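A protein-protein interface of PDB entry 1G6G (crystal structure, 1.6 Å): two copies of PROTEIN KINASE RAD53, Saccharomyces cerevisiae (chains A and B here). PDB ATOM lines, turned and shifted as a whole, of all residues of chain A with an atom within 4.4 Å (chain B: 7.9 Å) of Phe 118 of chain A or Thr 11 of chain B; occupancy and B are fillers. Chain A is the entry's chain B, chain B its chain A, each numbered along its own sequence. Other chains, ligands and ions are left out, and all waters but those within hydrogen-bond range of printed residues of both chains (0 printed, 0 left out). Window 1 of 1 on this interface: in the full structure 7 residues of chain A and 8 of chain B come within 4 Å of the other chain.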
ATOM      1  N   CYS A   6       8.686 -20.840 -13.550  1.00  0.00           N
ATOM      2  CA  CYS A   6       7.928 -20.718 -12.313  1.00  0.00           C
ATOM      3  C   CYS A   6       8.768 -20.170 -11.174  1.00  0.00           C
ATOM      4  O   CYS A   6      10.007 -20.178 -11.222  1.00  0.00           O
ATOM      5  CB  CYS A   6       7.305 -22.059 -11.916  1.00  0.00           C
ATOM      6  SG  CYS A   6       8.499 -23.348 -11.523  1.00  0.00           S
ATOM      7  N   ARG A   7       8.069 -19.643 -10.172  1.00  0.00           N
ATOM      8  CA  ARG A   7       8.688 -19.182  -8.936  1.00  0.00           C
ATOM      9  C   ARG A   7       8.357 -20.141  -7.780  1.00  0.00           C
ATOM     10  O   ARG A   7       7.214 -20.563  -7.608  1.00  0.00           O
ATOM     11  CB  ARG A   7       8.268 -17.747  -8.577  1.00  0.00           C
ATOM     12  CG  ARG A   7       8.825 -17.307  -7.223  1.00  0.00           C
ATOM     13  CD  ARG A   7       8.881 -15.793  -7.048  1.00  0.00           C
ATOM     14  NE  ARG A   7       9.823 -15.207  -7.995  1.00  0.00           N
ATOM     15  CZ  ARG A   7      10.114 -13.911  -8.021  1.00  0.00           C
ATOM     16  NH1 ARG A   7       9.522 -13.083  -7.161  1.00  0.00           N
ATOM     17  NH2 ARG A   7      10.990 -13.442  -8.893  1.00  0.00           N
ATOM     18  N   ILE A   9       8.188 -20.440  -3.860  1.00  0.00           N
ATOM     19  CA  ILE A   9       8.123 -19.679  -2.624  1.00  0.00           C
ATOM     20  C   ILE A   9       8.157 -20.662  -1.470  1.00  0.00           C
ATOM     21  O   ILE A   9       7.230 -21.433  -1.322  1.00  0.00           O
ATOM     22  CB  ILE A   9       6.811 -18.878  -2.547  1.00  0.00           C
ATOM     23  CG1 ILE A   9       6.714 -17.934  -3.740  1.00  0.00           C
ATOM     24  CG2 ILE A   9       6.742 -18.077  -1.218  1.00  0.00           C
ATOM     25  CD1 ILE A   9       5.938 -16.703  -3.456  1.00  0.00           C
ATOM     26  N   ILE A  17      13.515 -16.893  -2.196  1.00  0.00           N
ATOM     27  CA  ILE A  17      12.800 -17.055  -3.441  1.00  0.00           C
ATOM     28  C   ILE A  17      13.747 -17.466  -4.538  1.00  0.00           C
ATOM     29  O   ILE A  17      14.837 -16.914  -4.663  1.00  0.00           O
ATOM     30  CB  ILE A  17      12.141 -15.733  -3.817  1.00  0.00           C
ATOM     31  CG1 ILE A  17      10.976 -15.460  -2.877  1.00  0.00           C
ATOM     32  CG2 ILE A  17      11.674 -15.763  -5.245  1.00  0.00           C
ATOM     33  CD1 ILE A  17      10.437 -14.066  -3.025  1.00  0.00           C
ATOM     34  N   GLN A  98      -1.386 -24.091 -10.323  1.00  0.00           N
ATOM     35  CA  GLN A  98      -1.033 -22.822  -9.705  1.00  0.00           C
ATOM     36  C   GLN A  98      -1.306 -22.781  -8.209  1.00  0.00           C
ATOM     37  O   GLN A  98      -2.409 -23.103  -7.751  1.00  0.00           O
ATOM     38  CB  GLN A  98      -1.742 -21.652 -10.403  1.00  0.00           C
ATOM     39  CG  GLN A  98      -1.336 -20.297  -9.863  1.00  0.00           C
ATOM     40  CD  GLN A  98      -0.030 -19.833 -10.447  1.00  0.00           C
ATOM     41  OE1 GLN A  98       1.028 -20.367 -10.125  1.00  0.00           O
ATOM     42  NE2 GLN A  98      -0.098 -18.846 -11.332  1.00  0.00           N
ATOM     43  N   GLY A  99      -0.285 -22.385  -7.457  1.00  0.00           N
ATOM     44  CA  GLY A  99      -0.372 -22.271  -6.018  1.00  0.00           C
ATOM     45  C   GLY A  99      -0.234 -23.584  -5.270  1.00  0.00           C
ATOM     46  O   GLY A  99      -0.372 -23.613  -4.046  1.00  0.00           O
ATOM     47  N   VAL A 116       5.490 -23.368  -2.297  1.00  0.00           N
ATOM     48  CA  VAL A 116       4.357 -23.122  -3.178  1.00  0.00           C
ATOM     49  C   VAL A 116       4.892 -22.717  -4.537  1.00  0.00           C
ATOM     50  O   VAL A 116       5.840 -21.923  -4.629  1.00  0.00           O
ATOM     51  CB  VAL A 116       3.425 -22.012  -2.634  1.00  0.00           C
ATOM     52  CG1 VAL A 116       2.361 -21.662  -3.662  1.00  0.00           C
ATOM     53  CG2 VAL A 116       2.797 -22.454  -1.305  1.00  0.00           C
ATOM     54  N   ILE A 117       4.311 -23.286  -5.587  1.00  0.00           N
ATOM     55  CA  ILE A 117       4.754 -23.046  -6.941  1.00  0.00           C
ATOM     56  C   ILE A 117       3.878 -22.004  -7.589  1.00  0.00           C
ATOM     57  O   ILE A 117       2.650 -22.098  -7.527  1.00  0.00           O
ATOM     58  CB  ILE A 117       4.686 -24.349  -7.758  1.00  0.00           C
ATOM     59  CG1 ILE A 117       5.499 -25.430  -7.054  1.00  0.00           C
ATOM     60  CG2 ILE A 117       5.205 -24.130  -9.175  1.00  0.00           C
ATOM     61  CD1 ILE A 117       6.971 -25.129  -7.029  1.00  0.00           C
ATOM     62  N   PHE A 118       4.522 -21.004  -8.202  1.00  0.00           N
ATOM     63  CA  PHE A 118       3.831 -19.979  -8.965  1.00  0.00           C
ATOM     64  C   PHE A 118       4.343 -20.038 -10.377  1.00  0.00           C
ATOM     65  O   PHE A 118       5.519 -19.826 -10.639  1.00  0.00           O
ATOM     66  CB  PHE A 118       3.988 -18.593  -8.340  1.00  0.00           C
ATOM     67  CG  PHE A 118       3.260 -18.476  -7.065  1.00  0.00           C
ATOM     68  CD1 PHE A 118       3.916 -18.636  -5.865  1.00  0.00           C
ATOM     69  CD2 PHE A 118       1.890 -18.305  -7.063  1.00  0.00           C
ATOM     70  CE1 PHE A 118       3.233 -18.560  -4.683  1.00  0.00           C
ATOM     71  CE2 PHE A 118       1.198 -18.232  -5.881  1.00  0.00           C
ATOM     72  CZ  PHE A 118       1.868 -18.362  -4.690  1.00  0.00           C
ATOM     73  N   ILE A 119       3.432 -20.394 -11.263  1.00  0.00           N
ATOM     74  CA  ILE A 119       3.734 -20.620 -12.649  1.00  0.00           C
ATOM     75  C   ILE A 119       3.680 -19.299 -13.423  1.00  0.00           C
ATOM     76  O   ILE A 119       2.741 -18.525 -13.246  1.00  0.00           O
ATOM     77  CB  ILE A 119       2.700 -21.622 -13.216  1.00  0.00           C
ATOM     78  CG1 ILE A 119       2.752 -22.941 -12.432  1.00  0.00           C
ATOM     79  CG2 ILE A 119       2.921 -21.847 -14.685  1.00  0.00           C
ATOM     80  CD1 ILE A 119       1.562 -23.849 -12.690  1.00  0.00           C
ATOM     81  N   ASN A 120       4.707 -19.048 -14.232  1.00  0.00           N
ATOM     82  CA  ASN A 120       4.722 -17.887 -15.119  1.00  0.00           C
ATOM     83  C   ASN A 120       3.911 -18.174 -16.382  1.00  0.00           C
ATOM     84  O   ASN A 120       4.383 -18.869 -17.269  1.00  0.00           O
ATOM     85  CB  ASN A 120       6.157 -17.532 -15.502  1.00  0.00           C
ATOM     86  CG  ASN A 120       6.219 -16.357 -16.460  1.00  0.00           C
ATOM     87  OD1 ASN A 120       5.219 -15.680 -16.666  1.00  0.00           O
ATOM     88  ND2 ASN A 120       7.389 -16.112 -17.035  1.00  0.00           N
ATOM     89  N   VAL B   8      -3.786 -15.235   1.068  1.00  0.00           N
ATOM     90  CA  VAL B   8      -3.040 -14.250   0.293  1.00  0.00           C
ATOM     91  C   VAL B   8      -1.574 -14.619   0.358  1.00  0.00           C
ATOM     92  O   VAL B   8      -0.970 -14.618   1.444  1.00  0.00           O
ATOM     93  CB  VAL B   8      -3.213 -12.827   0.877  1.00  0.00           C
ATOM     94  CG1 VAL B   8      -2.452 -11.800   0.042  1.00  0.00           C
ATOM     95  CG2 VAL B   8      -4.686 -12.438   0.959  1.00  0.00           C
ATOM     96  N   ILE B   9      -0.999 -14.952  -0.792  1.00  0.00           N
ATOM     97  CA  ILE B   9       0.421 -15.306  -0.813  1.00  0.00           C
ATOM     98  C   ILE B   9       1.215 -14.218  -1.530  1.00  0.00           C
ATOM     99  O   ILE B   9       0.969 -13.909  -2.704  1.00  0.00           O
ATOM    100  CB  ILE B   9       0.641 -16.667  -1.470  1.00  0.00           C
ATOM    101  CG1 ILE B   9      -0.274 -17.703  -0.790  1.00  0.00           C
ATOM    102  CG2 ILE B   9       2.104 -17.075  -1.386  1.00  0.00           C
ATOM    103  CD1 ILE B   9      -0.002 -19.145  -1.187  1.00  0.00           C
ATOM    104  N   CYS B  10       2.152 -13.592  -0.802  1.00  0.00           N
ATOM    105  CA  CYS B  10       3.013 -12.592  -1.438  1.00  0.00           C
ATOM    106  C   CYS B  10       4.137 -13.305  -2.205  1.00  0.00           C
ATOM    107  O   CYS B  10       4.876 -14.144  -1.628  1.00  0.00           O
ATOM    108  CB  CYS B  10       3.557 -11.644  -0.354  1.00  0.00           C
ATOM    109  SG  CYS B  10       4.830 -10.498  -0.959  1.00  0.00           S
ATOM    110  N   THR B  11       4.258 -13.012  -3.503  1.00  0.00           N
ATOM    111  CA  THR B  11       5.237 -13.682  -4.351  1.00  0.00           C
ATOM    112  C   THR B  11       6.547 -12.947  -4.486  1.00  0.00           C
ATOM    113  O   THR B  11       7.460 -13.464  -5.141  1.00  0.00           O
ATOM    114  CB  THR B  11       4.703 -13.895  -5.769  1.00  0.00           C
ATOM    115  OG1 THR B  11       4.275 -12.623  -6.304  1.00  0.00           O
ATOM    116  CG2 THR B  11       3.449 -14.794  -5.735  1.00  0.00           C
ATOM    117  N   THR B  12       6.633 -11.738  -3.936  1.00  0.00           N
ATOM    118  CA  THR B  12       7.815 -10.904  -4.136  1.00  0.00           C
ATOM    119  C   THR B  12       8.741 -10.820  -2.914  1.00  0.00           C
ATOM    120  O   THR B  12       9.757 -10.095  -2.941  1.00  0.00           O
ATOM    121  CB  THR B  12       7.384  -9.502  -4.647  1.00  0.00           C
ATOM    122  OG1 THR B  12       6.281  -9.028  -3.858  1.00  0.00           O
ATOM    123  CG2 THR B  12       6.855  -9.631  -6.097  1.00  0.00           C
ATOM    124  N   GLY B  13       8.381 -11.553  -1.868  1.00  0.00           N
ATOM    125  CA  GLY B  13       9.254 -11.732  -0.720  1.00  0.00           C
ATOM    126  C   GLY B  13       9.103 -10.884   0.522  1.00  0.00           C
ATOM    127  O   GLY B  13       9.724 -11.201   1.552  1.00  0.00           O
ATOM    128  N   GLN B  14       8.277  -9.845   0.479  1.00  0.00           N
ATOM    129  CA  GLN B  14       8.212  -8.943   1.619  1.00  0.00           C
ATOM    130  C   GLN B  14       7.377  -9.410   2.790  1.00  0.00           C
ATOM    131  O   GLN B  14       7.622  -9.001   3.916  1.00  0.00           O
ATOM    132  CB  GLN B  14       7.707  -7.559   1.190  1.00  0.00           C
ATOM    133  CG  GLN B  14       8.521  -6.873   0.086  1.00  0.00           C
ATOM    134  CD  GLN B  14       7.959  -7.109  -1.309  1.00  0.00           C
ATOM    135  OE1 GLN B  14       7.458  -8.202  -1.606  1.00  0.00           O
ATOM    136  NE2 GLN B  14       8.057  -6.098  -2.170  1.00  0.00           N
ATOM    137  N   ILE B  15       6.378 -10.250   2.523  1.00  0.00           N
ATOM    138  CA  ILE B  15       5.379 -10.600   3.523  1.00  0.00           C
ATOM    139  C   ILE B  15       5.070 -12.098   3.517  1.00  0.00           C
ATOM    140  O   ILE B  15       4.972 -12.698   2.462  1.00  0.00           O
ATOM    141  CB  ILE B  15       4.071  -9.819   3.194  1.00  0.00           C
ATOM    142  CG1 ILE B  15       4.368  -8.324   3.019  1.00  0.00           C
ATOM    143  CG2 ILE B  15       3.022 -10.071   4.254  1.00  0.00           C
ATOM    144  CD1 ILE B  15       3.149  -7.503   2.650  1.00  0.00           C
ATOM    145  N   ILE B  17       2.702 -15.641   4.304  1.00  0.00           N
ATOM    146  CA  ILE B  17       1.301 -15.933   3.967  1.00  0.00           C
ATOM    147  C   ILE B  17       0.367 -15.401   5.052  1.00  0.00           C
ATOM    148  O   ILE B  17       0.673 -15.469   6.253  1.00  0.00           O
ATOM    149  CB  ILE B  17       1.140 -17.453   3.791  1.00  0.00           C
ATOM    150  CG1 ILE B  17       1.895 -17.893   2.547  1.00  0.00           C
ATOM    151  CG2 ILE B  17      -0.370 -17.840   3.772  1.00  0.00           C
ATOM    152  CD1 ILE B  17       1.766 -19.375   2.199  1.00  0.00           C
ATOM    153  N   TYR B  48      -4.384  -5.604   6.326  1.00  0.00           N
ATOM    154  CA  TYR B  48      -3.210  -6.191   5.700  1.00  0.00           C
ATOM    155  C   TYR B  48      -2.233  -5.051   5.451  1.00  0.00           C
ATOM    156  O   TYR B  48      -2.506  -4.142   4.670  1.00  0.00           O
ATOM    157  CB  TYR B  48      -3.612  -6.863   4.391  1.00  0.00           C
ATOM    158  CG  TYR B  48      -2.501  -7.656   3.723  1.00  0.00           C
ATOM    159  CD1 TYR B  48      -2.515  -9.057   3.750  1.00  0.00           C
ATOM    160  CD2 TYR B  48      -1.466  -7.017   3.043  1.00  0.00           C
ATOM    161  CE1 TYR B  48      -1.525  -9.795   3.107  1.00  0.00           C
ATOM    162  CE2 TYR B  48      -0.497  -7.730   2.375  1.00  0.00           C
ATOM    163  CZ  TYR B  48      -0.506  -9.133   2.434  1.00  0.00           C
ATOM    164  OH  TYR B  48       0.474  -9.842   1.793  1.00  0.00           O
ATOM    165  N   GLY B  99      -6.626 -17.565  -8.028  1.00  0.00           N
ATOM    166  CA  GLY B  99      -5.304 -17.378  -8.585  1.00  0.00           C
ATOM    167  C   GLY B  99      -5.002 -15.998  -9.140  1.00  0.00           C
ATOM    168  O   GLY B  99      -3.950 -15.786  -9.709  1.00  0.00           O
ATOM    169  N   ASP B 100      -5.937 -15.059  -8.990  1.00  0.00           N
ATOM    170  CA  ASP B 100      -5.705 -13.706  -9.489  1.00  0.00           C
ATOM    171  C   ASP B 100      -4.514 -13.089  -8.771  1.00  0.00           C
ATOM    172  O   ASP B 100      -4.318 -13.323  -7.563  1.00  0.00           O
ATOM    173  CB  ASP B 100      -6.912 -12.818  -9.217  1.00  0.00           C
ATOM    174  CG  ASP B 100      -7.974 -12.887 -10.311  1.00  0.00           C
ATOM    175  OD1 ASP B 100      -7.719 -13.476 -11.398  1.00  0.00           O
ATOM    176  OD2 ASP B 100      -9.072 -12.320 -10.136  1.00  0.00           O
ATOM    177  N   GLU B 101      -3.761 -12.301  -9.524  1.00  0.00           N
ATOM    178  CA  GLU B 101      -2.563 -11.617  -9.013  1.00  0.00           C
ATOM    179  C   GLU B 101      -2.849 -10.138  -8.832  1.00  0.00           C
ATOM    180  O   GLU B 101      -3.245  -9.471  -9.782  1.00  0.00           O
ATOM    181  CB  GLU B 101      -1.402 -11.799  -9.980  1.00  0.00           C
ATOM    182  CG  GLU B 101      -0.102 -11.147  -9.505  1.00  0.00           C
ATOM    183  CD  GLU B 101       1.116 -11.501 -10.351  1.00  0.00           C
ATOM    184  OE1 GLU B 101       0.959 -12.065 -11.470  1.00  0.00           O
ATOM    185  OE2 GLU B 101       2.243 -11.159  -9.932  1.00  0.00           O
ATOM    186  N   ILE B 102      -2.690  -9.632  -7.604  1.00  0.00           N
ATOM    187  CA  ILE B 102      -2.941  -8.212  -7.339  1.00  0.00           C
ATOM    188  C   ILE B 102      -1.590  -7.562  -7.064  1.00  0.00           C
ATOM    189  O   ILE B 102      -0.842  -8.067  -6.225  1.00  0.00           O
ATOM    190  CB  ILE B 102      -3.870  -8.038  -6.115  1.00  0.00           C
ATOM    191  CG1 ILE B 102      -5.226  -8.709  -6.372  1.00  0.00           C
ATOM    192  CG2 ILE B 102      -4.062  -6.519  -5.834  1.00  0.00           C
ATOM    193  CD1 ILE B 102      -6.171  -8.676  -5.182  1.00  0.00           C
ATOM    194  N   THR B 103      -1.280  -6.449  -7.732  1.00  0.00           N
ATOM    195  CA  THR B 103       0.070  -5.882  -7.612  1.00  0.00           C
ATOM    196  C   THR B 103       0.019  -4.393  -7.365  1.00  0.00           C
ATOM    197  O   THR B 103      -0.818  -3.688  -7.952  1.00  0.00           O
ATOM    198  CB  THR B 103       0.849  -6.127  -8.940  1.00  0.00           C
ATOM    199  OG1 THR B 103       0.771  -7.532  -9.276  1.00  0.00           O
ATOM    200  CG2 THR B 103       2.372  -5.785  -8.774  1.00  0.00           C
ATOM    201  N   ILE B 112       7.746  -2.874  -6.214  1.00  0.00           N
ATOM    202  CA  ILE B 112       6.697  -3.816  -6.631  1.00  0.00           C
ATOM    203  C   ILE B 112       6.435  -4.835  -5.544  1.00  0.00           C
ATOM    204  O   ILE B 112       7.355  -5.487  -5.059  1.00  0.00           O
ATOM    205  CB  ILE B 112       7.064  -4.516  -7.960  1.00  0.00           C
ATOM    206  CG1 ILE B 112       7.030  -3.510  -9.112  1.00  0.00           C
ATOM    207  CG2 ILE B 112       6.106  -5.688  -8.245  1.00  0.00           C
ATOM    208  CD1 ILE B 112       7.407  -4.109 -10.434  1.00  0.00           C
ATOM    209  N   LEU B 113       5.174  -4.942  -5.141  1.00  0.00           N
ATOM    210  CA  LEU B 113       4.738  -5.921  -4.150  1.00  0.00           C
ATOM    211  C   LEU B 113       3.564  -6.650  -4.812  1.00  0.00           C
ATOM    212  O   LEU B 113       2.573  -6.019  -5.168  1.00  0.00           O
ATOM    213  CB  LEU B 113       4.314  -5.215  -2.850  1.00  0.00           C
ATOM    214  CG  LEU B 113       4.051  -6.121  -1.645  1.00  0.00           C
ATOM    215  CD1 LEU B 113       4.097  -5.303  -0.324  1.00  0.00           C
ATOM    216  CD2 LEU B 113       2.706  -6.783  -1.840  1.00  0.00           C
ATOM    217  N   SER B 114       3.689  -7.966  -5.017  1.00  0.00           N
ATOM    218  CA  SER B 114       2.651  -8.729  -5.715  1.00  0.00           C
ATOM    219  C   SER B 114       2.073  -9.848  -4.844  1.00  0.00           C
ATOM    220  O   SER B 114       2.783 -10.488  -4.062  1.00  0.00           O
ATOM    221  CB  SER B 114       3.180  -9.266  -7.054  1.00  0.00           C
ATOM    222  OG  SER B 114       2.070  -9.489  -7.929  1.00  0.00           O
ATOM    223  N   LEU B 115       0.765 -10.075  -4.984  1.00  0.00           N
ATOM    224  CA  LEU B 115       0.027 -10.978  -4.125  1.00  0.00           C
ATOM    225  C   LEU B 115      -0.823 -11.865  -4.998  1.00  0.00           C
ATOM    226  O   LEU B 115      -1.368 -11.400  -6.007  1.00  0.00           O
ATOM    227  CB  LEU B 115      -0.905 -10.174  -3.213  1.00  0.00           C
ATOM    228  CG  LEU B 115      -0.310  -9.013  -2.426  1.00  0.00           C
ATOM    229  CD1 LEU B 115      -1.442  -8.227  -1.768  1.00  0.00           C
ATOM    230  CD2 LEU B 115       0.676  -9.547  -1.395  1.00  0.00           C
ATOM    231  N   VAL B 116      -0.941 -13.127  -4.624  1.00  0.00           N
ATOM    232  CA  VAL B 116      -1.814 -14.034  -5.368  1.00  0.00           C
ATOM    233  C   VAL B 116      -2.903 -14.521  -4.411  1.00  0.00           C
ATOM    234  O   VAL B 116      -2.637 -14.884  -3.262  1.00  0.00           O
ATOM    235  CB  VAL B 116      -1.038 -15.201  -6.007  1.00  0.00           C
ATOM    236  CG1 VAL B 116      -2.009 -16.180  -6.691  1.00  0.00           C
ATOM    237  CG2 VAL B 116      -0.030 -14.629  -7.014  1.00  0.00           C
ATOM    238  N   ILE B 117      -4.157 -14.484  -4.865  1.00  0.00           N
ATOM    239  CA  ILE B 117      -5.281 -14.862  -4.003  1.00  0.00           C
ATOM    240  C   ILE B 117      -5.794 -16.266  -4.298  1.00  0.00           C
ATOM    241  O   ILE B 117      -6.024 -16.617  -5.476  1.00  0.00           O
ATOM    242  CB  ILE B 117      -6.469 -13.884  -4.214  1.00  0.00           C
ATOM    243  CG1 ILE B 117      -6.013 -12.435  -4.132  1.00  0.00           C
ATOM    244  CG2 ILE B 117      -7.590 -14.146  -3.210  1.00  0.00           C
ATOM    245  CD1 ILE B 117      -5.736 -11.968  -2.731  1.00  0.00           C
ATOM    246  N   PHE B 118      -5.953 -17.054  -3.245  1.00  0.00           N
ATOM    247  CA  PHE B 118      -6.585 -18.362  -3.363  1.00  0.00           C
ATOM    248  C   PHE B 118      -7.848 -18.352  -2.528  1.00  0.00           C
ATOM    249  O   PHE B 118      -7.829 -18.118  -1.329  1.00  0.00           O
ATOM    250  CB  PHE B 118      -5.614 -19.465  -2.975  1.00  0.00           C
ATOM    251  CG  PHE B 118      -4.422 -19.496  -3.858  1.00  0.00           C
ATOM    252  CD1 PHE B 118      -3.247 -18.887  -3.462  1.00  0.00           C
ATOM    253  CD2 PHE B 118      -4.497 -20.065  -5.125  1.00  0.00           C
ATOM    254  CE1 PHE B 118      -2.140 -18.883  -4.295  1.00  0.00           C
ATOM    255  CE2 PHE B 118      -3.396 -20.054  -5.961  1.00  0.00           C
ATOM    256  CZ  PHE B 118      -2.216 -19.456  -5.536  1.00  0.00           C
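The backbone carbonyl oxygen (O) of Thr 11 of chain B sits at hydrogen-bond distance from the guanidinium group (NH1) of Arg 7 of chain A (2.9 Å).
Gly 99 of chain A touches Phe 118 of chain B, but with the chains exchanged Phe 118 of chain A does not touch Gly 99 of chain B (6.9 Å). Phe 118 of chain A touches Ile 9 of chain B, but with the chains exchanged Ile 9 of chain A does not touch Phe 118 of chain B (8.4 Å). Phe 118 of chain A touches Val 116 of chain B, but with the chains exchanged Val 116 of chain A does not touch Phe 118 of chain B (5.3 Å). Phe 118 of chain A touches its own counterpart, Phe 118 of chain B. Positions printed for both chains: 9, 17, 99, 116, 117 and 118. Of the 12 pairs that touch across the chains among the printed residues, 1 has its exchanged pair printed and touching as well.
Of the printed residues of chain B, Arg 7 of chain A touches Thr 11 (2.9 Å). Printed residues of chain B within 4 Å of Phe 118 of chain A: Ile 9 (3.6 Å), Thr 11 (3.9 Å), Val 116 (3.8 Å) and Phe 118 (3.6 Å). Printed residues of chain A within 4 Å of Cys 10 of chain B: Ile 9 (3.3 Å). Of the printed residues of chain A, Thr 11 of chain B touches Arg 7, Ile 9, Ile 17 and Phe 118. Ile 15 of chain B touches none of the printed residues of chain A. Printed residues of chain A within 4 Å of Val 116 of chain B: Phe 118 (3.8 Å).
The backbone NH (N) of Val 116 of chain B sits at hydrogen-bond distance from the backbone carbonyl oxygen (O) of Ile 9 of chain B (2.8 Å). The side-chain amide oxygen (OE1) of Gln 14 of chain B sits at hydrogen-bond distance from the side-chain sulfur (SG) of Cys 10 of chain B (3.5 Å). O of Ser 114 of chain B lies close to SG of Cys 10 of chain B, 3.7 Å away. N of Arg 7 of chain A is in hydrogen-bond range of O of Phe 118 of chain A, 2.6 Å away. The side-chain amide oxygen (OE1) of Gln 98 of chain A is in hydrogen-bond range of the backbone NH (N) of Ile 119 of chain A (2.7 Å). The backbone NH of Gly 99 of chain A lies within hydrogen-bond range of the backbone carbonyl oxygen of Ile 117 of chain A, at 2.9 Å.
Ile 9 of chain A touches Cys 10 of chain B. CA of Thr 11 of chain B touches CD1 of Ile 9 of chain A, 3.2 Å away. O of Thr 11 of chain B touches CD1 of Ile 17 of chain A (3.7 Å). Thr 12 of chain B touches Ile 17 of chain A. CD1 of Ile 17 of chain A touches N of Gly 13 of chain B, at 3.4 Å. CE2 of Phe 118 of chain B touches O of Gln 98 of chain A (3.7 Å). Ile 9 of chain B touches Phe 118 of chain A (CG2 to CZ, 3.6 Å). Phe 118 of chain A touches Thr 11 of chain B. Val 116 of chain B touches Phe 118 of chain A (CB to CE2, 3.8 Å). CZ of Phe 118 of chain B touches CE2 of Phe 118 of chain A, at 3.6 Å.
Hydrophobic or aromatic side chains of chain B within 4 Å of the printed part of chain A: Ile 9, Val 116 and Phe 118. Of the 11 printed residues of chain A, 6 touch a printed residue of chain B. Hydrophobic or aromatic side chains of chain A within 4 Å of the printed part of chain B: Ile 9, Ile 17 and Phe 118.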
